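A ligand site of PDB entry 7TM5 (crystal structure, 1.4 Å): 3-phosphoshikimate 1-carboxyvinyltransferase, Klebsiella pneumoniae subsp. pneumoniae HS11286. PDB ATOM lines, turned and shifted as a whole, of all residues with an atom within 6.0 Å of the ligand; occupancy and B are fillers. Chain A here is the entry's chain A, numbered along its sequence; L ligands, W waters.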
ATOM      1  N   LYS A  30      23.517 -16.456   8.198  1.00  0.00           N
ATOM      2  CA  LYS A  30      24.451 -16.197   7.110  1.00  0.00           C
ATOM      3  C   LYS A  30      24.070 -16.985   5.851  1.00  0.00           C
ATOM      4  O   LYS A  30      24.042 -16.442   4.728  1.00  0.00           O
ATOM      5  CB  LYS A  30      25.872 -16.539   7.544  1.00  0.00           C
ATOM      6  CG  LYS A  30      26.922 -16.383   6.440  1.00  0.00           C
ATOM      7  CD  LYS A  30      27.426 -17.760   5.899  1.00  0.00           C
ATOM      8  CE  LYS A  30      28.528 -18.338   6.789  1.00  0.00           C
ATOM      9  NZ  LYS A  30      28.768 -19.781   6.541  1.00  0.00           N
ATOM     10  N   SER A  31      23.772 -18.279   6.020  1.00  0.00           N
ATOM     11  CA  SER A  31      23.452 -19.139   4.868  1.00  0.00           C
ATOM     12  C   SER A  31      22.225 -18.623   4.118  1.00  0.00           C
ATOM     13  O   SER A  31      22.202 -18.544   2.880  1.00  0.00           O
ATOM     14  CB  SER A  31      23.209 -20.563   5.365  1.00  0.00           C
ATOM     15  OG  SER A  31      24.383 -21.162   5.880  1.00  0.00           O
ATOM     16  N   VAL A  32      21.181 -18.281   4.870  1.00  0.00           N
ATOM     17  CA  VAL A  32      19.973 -17.766   4.234  1.00  0.00           C
ATOM     18  C   VAL A  32      20.234 -16.382   3.634  1.00  0.00           C
ATOM     19  O   VAL A  32      19.790 -16.081   2.525  1.00  0.00           O
ATOM     20  CB  VAL A  32      18.784 -17.749   5.220  1.00  0.00           C
ATOM     21  CG1 VAL A  32      17.588 -17.015   4.598  1.00  0.00           C
ATOM     22  CG2 VAL A  32      18.418 -19.168   5.678  1.00  0.00           C
ATOM     23  N   ARG A  35      22.162 -16.550   0.228  1.00  0.00           N
ATOM     24  CA  ARG A  35      21.298 -17.082  -0.824  1.00  0.00           C
ATOM     25  C   ARG A  35      20.215 -16.078  -1.218  1.00  0.00           C
ATOM     26  O   ARG A  35      19.968 -15.847  -2.411  1.00  0.00           O
ATOM     27  CB  ARG A  35      20.626 -18.357  -0.357  1.00  0.00           C
ATOM     28  CG  ARG A  35      21.511 -19.589  -0.318  1.00  0.00           C
ATOM     29  CD  ARG A  35      20.841 -20.653   0.512  1.00  0.00           C
ATOM     30  NE  ARG A  35      21.551 -21.923   0.494  1.00  0.00           N
ATOM     31  CZ  ARG A  35      22.626 -22.197   1.208  1.00  0.00           C
ATOM     32  NH1 ARG A  35      23.225 -21.277   1.961  1.00  0.00           N
ATOM     33  NH2 ARG A  35      23.132 -23.423   1.164  1.00  0.00           N
ATOM     34  N   THR A 105      29.937 -18.843   0.816  1.00  0.00           N
ATOM     35  CA  THR A 105      28.600 -18.585   0.291  1.00  0.00           C
ATOM     36  C   THR A 105      28.547 -17.383  -0.644  1.00  0.00           C
ATOM     37  O   THR A 105      27.486 -17.125  -1.215  1.00  0.00           O
ATOM     38  CB  THR A 105      27.548 -18.414   1.393  1.00  0.00           C
ATOM     39  OG1 THR A 105      27.845 -17.276   2.196  1.00  0.00           O
ATOM     40  CG2 THR A 105      27.447 -19.688   2.255  1.00  0.00           C
ATOM     41  N   ARG A 108      31.464 -19.494  -3.941  1.00  0.00           N
ATOM     42  CA  ARG A 108      30.918 -20.608  -4.730  1.00  0.00           C
ATOM     43  C   ARG A 108      29.687 -20.167  -5.522  1.00  0.00           C
ATOM     44  O   ARG A 108      29.672 -20.344  -6.767  1.00  0.00           O
ATOM     45  CB  ARG A 108      30.696 -21.835  -3.835  1.00  0.00           C
ATOM     46  CG  ARG A 108      31.953 -22.672  -3.500  1.00  0.00           C
ATOM     47  CD  ARG A 108      32.880 -21.973  -2.505  1.00  0.00           C
ATOM     48  NE  ARG A 108      33.990 -22.825  -2.068  1.00  0.00           N
ATOM     49  CZ  ARG A 108      33.981 -23.573  -0.967  1.00  0.00           C
ATOM     50  NH1 ARG A 108      32.947 -23.579  -0.144  1.00  0.00           N
ATOM     51  NH2 ARG A 108      35.048 -24.314  -0.692  1.00  0.00           N
ATOM     52  N   ARG A 132      41.085 -22.998  -0.348  1.00  0.00           N
ATOM     53  CA  ARG A 132      39.834 -23.748  -0.173  1.00  0.00           C
ATOM     54  C   ARG A 132      39.326 -24.237  -1.515  1.00  0.00           C
ATOM     55  O   ARG A 132      39.275 -23.469  -2.487  1.00  0.00           O
ATOM     56  CB  ARG A 132      38.779 -22.881   0.514  1.00  0.00           C
ATOM     57  CG  ARG A 132      39.147 -22.592   1.969  1.00  0.00           C
ATOM     58  CD  ARG A 132      38.107 -21.791   2.686  1.00  0.00           C
ATOM     59  NE  ARG A 132      36.863 -22.538   2.811  1.00  0.00           N
ATOM     60  CZ  ARG A 132      35.704 -22.035   3.189  1.00  0.00           C
ATOM     61  NH1 ARG A 132      35.575 -20.749   3.488  1.00  0.00           N
ATOM     62  NH2 ARG A 132      34.644 -22.837   3.292  1.00  0.00           N
ATOM     63  N   VAL A 176      32.962 -33.239  -1.036  1.00  0.00           N
ATOM     64  CA  VAL A 176      33.798 -32.256  -0.364  1.00  0.00           C
ATOM     65  C   VAL A 176      32.996 -31.075   0.154  1.00  0.00           C
ATOM     66  O   VAL A 176      33.165 -30.654   1.296  1.00  0.00           O
ATOM     67  CB  VAL A 176      34.973 -31.807  -1.267  1.00  0.00           C
ATOM     68  CG1 VAL A 176      35.706 -30.635  -0.631  1.00  0.00           C
ATOM     69  CG2 VAL A 176      35.897 -32.979  -1.483  1.00  0.00           C
ATOM     70  N   SER A 177      32.126 -30.505  -0.675  1.00  0.00           N
ATOM     71  CA  SER A 177      31.275 -29.421  -0.209  1.00  0.00           C
ATOM     72  C   SER A 177      29.922 -29.476  -0.899  1.00  0.00           C
ATOM     73  O   SER A 177      29.856 -29.651  -2.114  1.00  0.00           O
ATOM     74  CB  SER A 177      31.895 -28.053  -0.518  1.00  0.00           C
ATOM     75  OG  SER A 177      31.065 -26.991  -0.060  1.00  0.00           O
ATOM     76  N   SER A 178      28.854 -29.275  -0.124  1.00  0.00           N
ATOM     77  CA  SER A 178      27.527 -29.086  -0.716  1.00  0.00           C
ATOM     78  C   SER A 178      27.420 -27.744  -1.431  1.00  0.00           C
ATOM     79  O   SER A 178      26.481 -27.553  -2.216  1.00  0.00           O
ATOM     80  CB  SER A 178      26.440 -29.166   0.360  1.00  0.00           C
ATOM     81  OG  SER A 178      26.419 -28.027   1.212  1.00  0.00           O
ATOM     82  N   GLN A 179      28.339 -26.818  -1.159  1.00  0.00           N
ATOM     83  CA  GLN A 179      28.218 -25.491  -1.744  1.00  0.00           C
ATOM     84  C   GLN A 179      28.388 -25.527  -3.249  1.00  0.00           C
ATOM     85  O   GLN A 179      27.876 -24.646  -3.935  1.00  0.00           O
ATOM     86  CB  GLN A 179      29.220 -24.527  -1.116  1.00  0.00           C
ATOM     87  CG  GLN A 179      28.935 -24.199   0.344  1.00  0.00           C
ATOM     88  CD  GLN A 179      29.720 -22.996   0.860  1.00  0.00           C
ATOM     89  OE1 GLN A 179      30.439 -22.339   0.115  1.00  0.00           O
ATOM     90  NE2 GLN A 179      29.553 -22.693   2.133  1.00  0.00           N
ATOM     91  N   THR A 182      24.929 -26.433  -4.410  1.00  0.00           N
ATOM     92  CA  THR A 182      24.084 -25.262  -4.174  1.00  0.00           C
ATOM     93  C   THR A 182      24.291 -24.198  -5.254  1.00  0.00           C
ATOM     94  O   THR A 182      23.329 -23.615  -5.779  1.00  0.00           O
ATOM     95  CB  THR A 182      24.379 -24.707  -2.780  1.00  0.00           C
ATOM     96  OG1 THR A 182      23.627 -25.438  -1.812  1.00  0.00           O
ATOM     97  CG2 THR A 182      24.043 -23.234  -2.675  1.00  0.00           C
ATOM     98  N   VAL A 204      27.773 -34.666   0.993  1.00  0.00           N
ATOM     99  CA  VAL A 204      27.914 -34.161   2.350  1.00  0.00           C
ATOM    100  C   VAL A 204      27.005 -32.960   2.554  1.00  0.00           C
ATOM    101  O   VAL A 204      26.557 -32.320   1.596  1.00  0.00           O
ATOM    102  CB  VAL A 204      29.384 -33.816   2.698  1.00  0.00           C
ATOM    103  CG1 VAL A 204      30.265 -35.058   2.539  1.00  0.00           C
ATOM    104  CG2 VAL A 204      29.893 -32.667   1.852  1.00  0.00           C
ATOM    105  N   SER A 205      26.744 -32.628   3.816  1.00  0.00           N
ATOM    106  CA  SER A 205      26.043 -31.388   4.189  1.00  0.00           C
ATOM    107  C   SER A 205      24.696 -31.269   3.478  1.00  0.00           C
ATOM    108  O   SER A 205      24.295 -30.179   3.043  1.00  0.00           O
ATOM    109  CB  SER A 205      26.935 -30.161   3.957  1.00  0.00           C
ATOM    110  OG  SER A 205      27.954 -30.129   4.942  1.00  0.00           O
ATOM    111  N   TYR A 208      22.102 -28.357   3.822  1.00  0.00           N
ATOM    112  CA  TYR A 208      22.310 -27.079   3.155  1.00  0.00           C
ATOM    113  C   TYR A 208      21.755 -27.090   1.734  1.00  0.00           C
ATOM    114  O   TYR A 208      21.336 -26.038   1.223  1.00  0.00           O
ATOM    115  CB  TYR A 208      23.791 -26.705   3.190  1.00  0.00           C
ATOM    116  CG  TYR A 208      24.246 -26.330   4.568  1.00  0.00           C
ATOM    117  CD1 TYR A 208      24.064 -25.046   5.066  1.00  0.00           C
ATOM    118  CD2 TYR A 208      24.870 -27.256   5.396  1.00  0.00           C
ATOM    119  CE1 TYR A 208      24.481 -24.700   6.355  1.00  0.00           C
ATOM    120  CE2 TYR A 208      25.300 -26.921   6.675  1.00  0.00           C
ATOM    121  CZ  TYR A 208      25.104 -25.647   7.147  1.00  0.00           C
ATOM    122  OH  TYR A 208      25.538 -25.325   8.405  1.00  0.00           O
ATOM    123  N   ILE A 211      18.241 -26.135   2.353  1.00  0.00           N
ATOM    124  CA  ILE A 211      18.092 -24.676   2.433  1.00  0.00           C
ATOM    125  C   ILE A 211      17.988 -24.082   1.040  1.00  0.00           C
ATOM    126  O   ILE A 211      17.118 -23.249   0.739  1.00  0.00           O
ATOM    127  CB  ILE A 211      19.251 -24.009   3.197  1.00  0.00           C
ATOM    128  CG1 ILE A 211      19.334 -24.502   4.631  1.00  0.00           C
ATOM    129  CG2 ILE A 211      19.106 -22.479   3.136  1.00  0.00           C
ATOM    130  CD1 ILE A 211      20.479 -23.874   5.437  1.00  0.00           C
ATOM    131  N   THR A 212      18.921 -24.471   0.166  1.00  0.00           N
ATOM    132  CA  THR A 212      18.930 -23.931  -1.188  1.00  0.00           C
ATOM    133  C   THR A 212      17.610 -24.176  -1.904  1.00  0.00           C
ATOM    134  O   THR A 212      17.049 -23.261  -2.517  1.00  0.00           O
ATOM    135  CB  THR A 212      20.089 -24.523  -1.957  1.00  0.00           C
ATOM    136  OG1 THR A 212      21.276 -24.132  -1.268  1.00  0.00           O
ATOM    137  CG2 THR A 212      20.106 -24.030  -3.402  1.00  0.00           C
ATOM    138  N   PRO A 320      27.690 -30.009  10.343  1.00  0.00           N
ATOM    139  CA  PRO A 320      29.152 -29.861  10.494  1.00  0.00           C
ATOM    140  C   PRO A 320      29.608 -28.615  11.245  1.00  0.00           C
ATOM    141  O   PRO A 320      30.664 -28.651  11.899  1.00  0.00           O
ATOM    142  CB  PRO A 320      29.645 -29.865   9.042  1.00  0.00           C
ATOM    143  CG  PRO A 320      28.465 -29.306   8.265  1.00  0.00           C
ATOM    144  CD  PRO A 320      27.277 -29.950   8.925  1.00  0.00           C
ATOM    145  N   ASP A 321      28.875 -27.503  11.155  1.00  0.00           N
ATOM    146  CA  ASP A 321      29.287 -26.284  11.845  1.00  0.00           C
ATOM    147  C   ASP A 321      28.904 -26.328  13.328  1.00  0.00           C
ATOM    148  O   ASP A 321      29.754 -26.121  14.195  1.00  0.00           O
ATOM    149  CB  ASP A 321      28.656 -25.040  11.205  1.00  0.00           C
ATOM    150  CG  ASP A 321      29.261 -24.664   9.888  1.00  0.00           C
ATOM    151  OD1 ASP A 321      30.271 -25.251   9.476  1.00  0.00           O
ATOM    152  OD2 ASP A 321      28.701 -23.744   9.253  1.00  0.00           O
ATOM    153  N   ASN A 344      35.267 -32.689   5.943  1.00  0.00           N
ATOM    154  CA  ASN A 344      35.428 -31.359   5.335  1.00  0.00           C
ATOM    155  C   ASN A 344      35.679 -30.250   6.354  1.00  0.00           C
ATOM    156  O   ASN A 344      35.934 -29.096   5.961  1.00  0.00           O
ATOM    157  CB  ASN A 344      34.312 -31.037   4.337  1.00  0.00           C
ATOM    158  CG  ASN A 344      33.002 -30.654   4.975  1.00  0.00           C
ATOM    159  OD1 ASN A 344      32.879 -30.502   6.193  1.00  0.00           O
ATOM    160  ND2 ASN A 344      32.001 -30.457   4.130  1.00  0.00           N
ATOM    161  N   LYS A 348      37.805 -25.922   5.478  1.00  0.00           N
ATOM    162  CA  LYS A 348      36.929 -24.748   5.787  1.00  0.00           C
ATOM    163  C   LYS A 348      37.776 -23.533   6.216  1.00  0.00           C
ATOM    164  O   LYS A 348      38.863 -23.360   5.713  1.00  0.00           O
ATOM    165  CB  LYS A 348      35.851 -25.239   6.754  1.00  0.00           C
ATOM    166  CG  LYS A 348      34.784 -26.018   5.990  1.00  0.00           C
ATOM    167  CD  LYS A 348      33.654 -26.609   6.795  1.00  0.00           C
ATOM    168  CE  LYS A 348      32.560 -27.106   5.879  1.00  0.00           C
ATOM    169  NZ  LYS A 348      31.481 -27.807   6.615  1.00  0.00           N
ATOM    170  N   GLU A 349      37.211 -22.692   7.082  1.00  0.00           N
ATOM    171  CA  GLU A 349      37.890 -21.448   7.453  1.00  0.00           C
ATOM    172  C   GLU A 349      39.326 -21.689   7.893  1.00  0.00           C
ATOM    173  O   GLU A 349      40.213 -20.862   7.635  1.00  0.00           O
ATOM    174  CB  GLU A 349      37.099 -20.761   8.560  1.00  0.00           C
ATOM    175  CG  GLU A 349      35.877 -19.977   8.098  1.00  0.00           C
ATOM    176  CD  GLU A 349      34.618 -20.802   7.857  1.00  0.00           C
ATOM    177  OE1 GLU A 349      34.671 -22.043   7.646  1.00  0.00           O
ATOM    178  OE2 GLU A 349      33.545 -20.161   7.863  1.00  0.00           O
ATOM    179  N   ARG A 352      39.828 -27.421  10.597  1.00  0.00           N
ATOM    180  CA  ARG A 352      39.206 -27.397  11.912  1.00  0.00           C
ATOM    181  C   ARG A 352      39.457 -28.674  12.712  1.00  0.00           C
ATOM    182  O   ARG A 352      39.379 -28.631  13.947  1.00  0.00           O
ATOM    183  CB  ARG A 352      37.713 -27.134  11.771  1.00  0.00           C
ATOM    184  CG  ARG A 352      37.395 -25.732  11.321  1.00  0.00           C
ATOM    185  CD  ARG A 352      35.966 -25.543  10.884  1.00  0.00           C
ATOM    186  NE  ARG A 352      35.578 -24.142  10.965  1.00  0.00           N
ATOM    187  CZ  ARG A 352      34.406 -23.674  10.567  1.00  0.00           C
ATOM    188  NH1 ARG A 352      33.511 -24.436   9.971  1.00  0.00           N
ATOM    189  NH2 ARG A 352      34.118 -22.391  10.774  1.00  0.00           N
ATOM    190  N   ARG A 394      34.357 -19.559  14.396  1.00  0.00           N
ATOM    191  CA  ARG A 394      33.779 -20.647  15.229  1.00  0.00           C
ATOM    192  C   ARG A 394      34.788 -21.143  16.259  1.00  0.00           C
ATOM    193  O   ARG A 394      34.356 -21.608  17.296  1.00  0.00           O
ATOM    194  CB  ARG A 394      33.218 -21.766  14.334  1.00  0.00           C
ATOM    195  CG  ARG A 394      32.123 -21.273  13.392  1.00  0.00           C
ATOM    196  CD  ARG A 394      31.134 -22.355  13.029  1.00  0.00           C
ATOM    197  NE  ARG A 394      30.239 -21.808  12.026  1.00  0.00           N
ATOM    198  CZ  ARG A 394      29.209 -21.019  12.285  1.00  0.00           C
ATOM    199  NH1 ARG A 394      28.885 -20.720  13.525  1.00  0.00           N
ATOM    200  NH2 ARG A 394      28.492 -20.544  11.287  1.00  0.00           N
HETATM  201  C1  LIG L   1      27.012 -23.721   4.050  1.00  0.00           C
HETATM  202  C2  LIG L   1      27.385 -24.989   3.835  1.00  0.00           C
HETATM  203  C3  LIG L   1      28.361 -25.748   4.687  1.00  0.00           C
HETATM  204  C4  LIG L   1      28.687 -24.965   5.961  1.00  0.00           C
HETATM  205  C5  LIG L   1      28.903 -23.506   5.638  1.00  0.00           C
HETATM  206  C6  LIG L   1      27.609 -22.891   5.151  1.00  0.00           C
HETATM  207  C7  LIG L   1      25.985 -23.156   3.188  1.00  0.00           C
HETATM  208  O1  LIG L   1      29.533 -26.076   3.923  1.00  0.00           O
HETATM  209  O2  LIG L   1      29.830 -25.504   6.618  1.00  0.00           O
HETATM  210  O3  LIG L   1      29.350 -22.794   6.793  1.00  0.00           O
HETATM  211  O4  LIG L   1      25.734 -23.685   2.133  1.00  0.00           O
HETATM  212  O5  LIG L   1      25.393 -22.160   3.550  1.00  0.00           O
HETATM  213  P1  LIG L   1      29.883 -27.532   3.280  1.00  0.00           P
HETATM  214  O6  LIG L   1      31.206 -27.333   2.602  1.00  0.00           O
HETATM  215  O7  LIG L   1      29.944 -28.474   4.460  1.00  0.00           O
HETATM  216  O8  LIG L   1      28.772 -27.853   2.315  1.00  0.00           O
HETATM  217  O   HOH W   1      33.769 -27.876   2.442  1.00  0.00           O
HETATM  218  O   HOH W   2      32.442 -23.587   6.511  1.00  0.00           O
HETATM  219  O   HOH W   3      32.297 -24.622   2.540  1.00  0.00           O
HETATM  220  O   HOH W   4      25.431 -25.708   0.260  1.00  0.00           O
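The backbone NH (N) of Ser 178 is in hydrogen-bond range of an oxygen (O8) of the ligand (2.8 Å).
The side-chain hydroxyl (OG) of Ser 178 is in hydrogen-bond range of an oxygen (O8) of the ligand (2.6 Å).
OG of Ser 205 lies within hydrogen-bond range of O7 of the ligand, 2.6 Å away.
O6 of the ligand sits at hydrogen-bond distance from OG of Ser 177.
An oxygen (O3) of the ligand lies within hydrogen-bond range of the side-chain carboxylate of Asp 321.
OG of Ser 31 lies within hydrogen-bond range of O5 of the ligand, 2.7 Å away.
NZ of Lys 348 is in salt-bridge range of O7 of the ligand (2.7 Å).
NH2 of Arg 35 is in salt-bridge range of O4 of the ligand, 2.8 Å away.
An oxygen (O7) of the ligand sits at hydrogen-bond distance from the side-chain amide nitrogen of Asn 344, at 2.9 Å.
NZ of Lys 30 lies within hydrogen-bond range of O3 of the ligand, 3.1 Å away.
The side-chain hydroxyl (OG) of Ser 177 sits at hydrogen-bond distance from the backbone NH (N) of Gln 179 (2.9 Å).
OD1 of Asp 321 is in salt-bridge range of NH1 of Arg 352, at 3.4 Å.
The guanidinium group (NE) of Arg 394 lies within salt-bridge range of the side-chain carboxylate (OD2) of Asp 321, 3.7 Å away.
The side-chain amino group (NZ) of Lys 348 lies within hydrogen-bond range of the side-chain amide oxygen (OD1) of Asn 344, at 3.1 Å.
O of Tyr 208 is in hydrogen-bond range of NH2 of Arg 35.
The side-chain hydroxyl (OG1) of Thr 212 lies within hydrogen-bond range of the guanidinium group (NE) of Arg 35.
The side-chain hydroxyl of Thr 212 lies within hydrogen-bond range of the backbone carbonyl oxygen of Tyr 208 (3.1 Å).
NH1 of Arg 108 lies within hydrogen-bond range of OE1 of Gln 179 (2.8 Å).
CG2 of Thr 105 touches O5 of the ligand, 3.5 Å away.
Gln 179 touches the ligand.
Tyr 208 touches the ligand (CD1 to C7, 3.3 Å).
The nearest printed residue that does not touch the ligand is Val 176 (4.1 Å).
Water W1 bridges O6 of the ligand (2.6 Å) and O of Val 176 (3.1 Å).
Water W4 lies within hydrogen-bond range of OG of Ser 178, OG1 of Thr 182, O4 of the ligand, NH2 of Arg 35 and N of Gln 179.
Water W2 bridges the side-chain carboxylate (OE1) of Glu 349 and an oxygen (O3) of the ligand.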
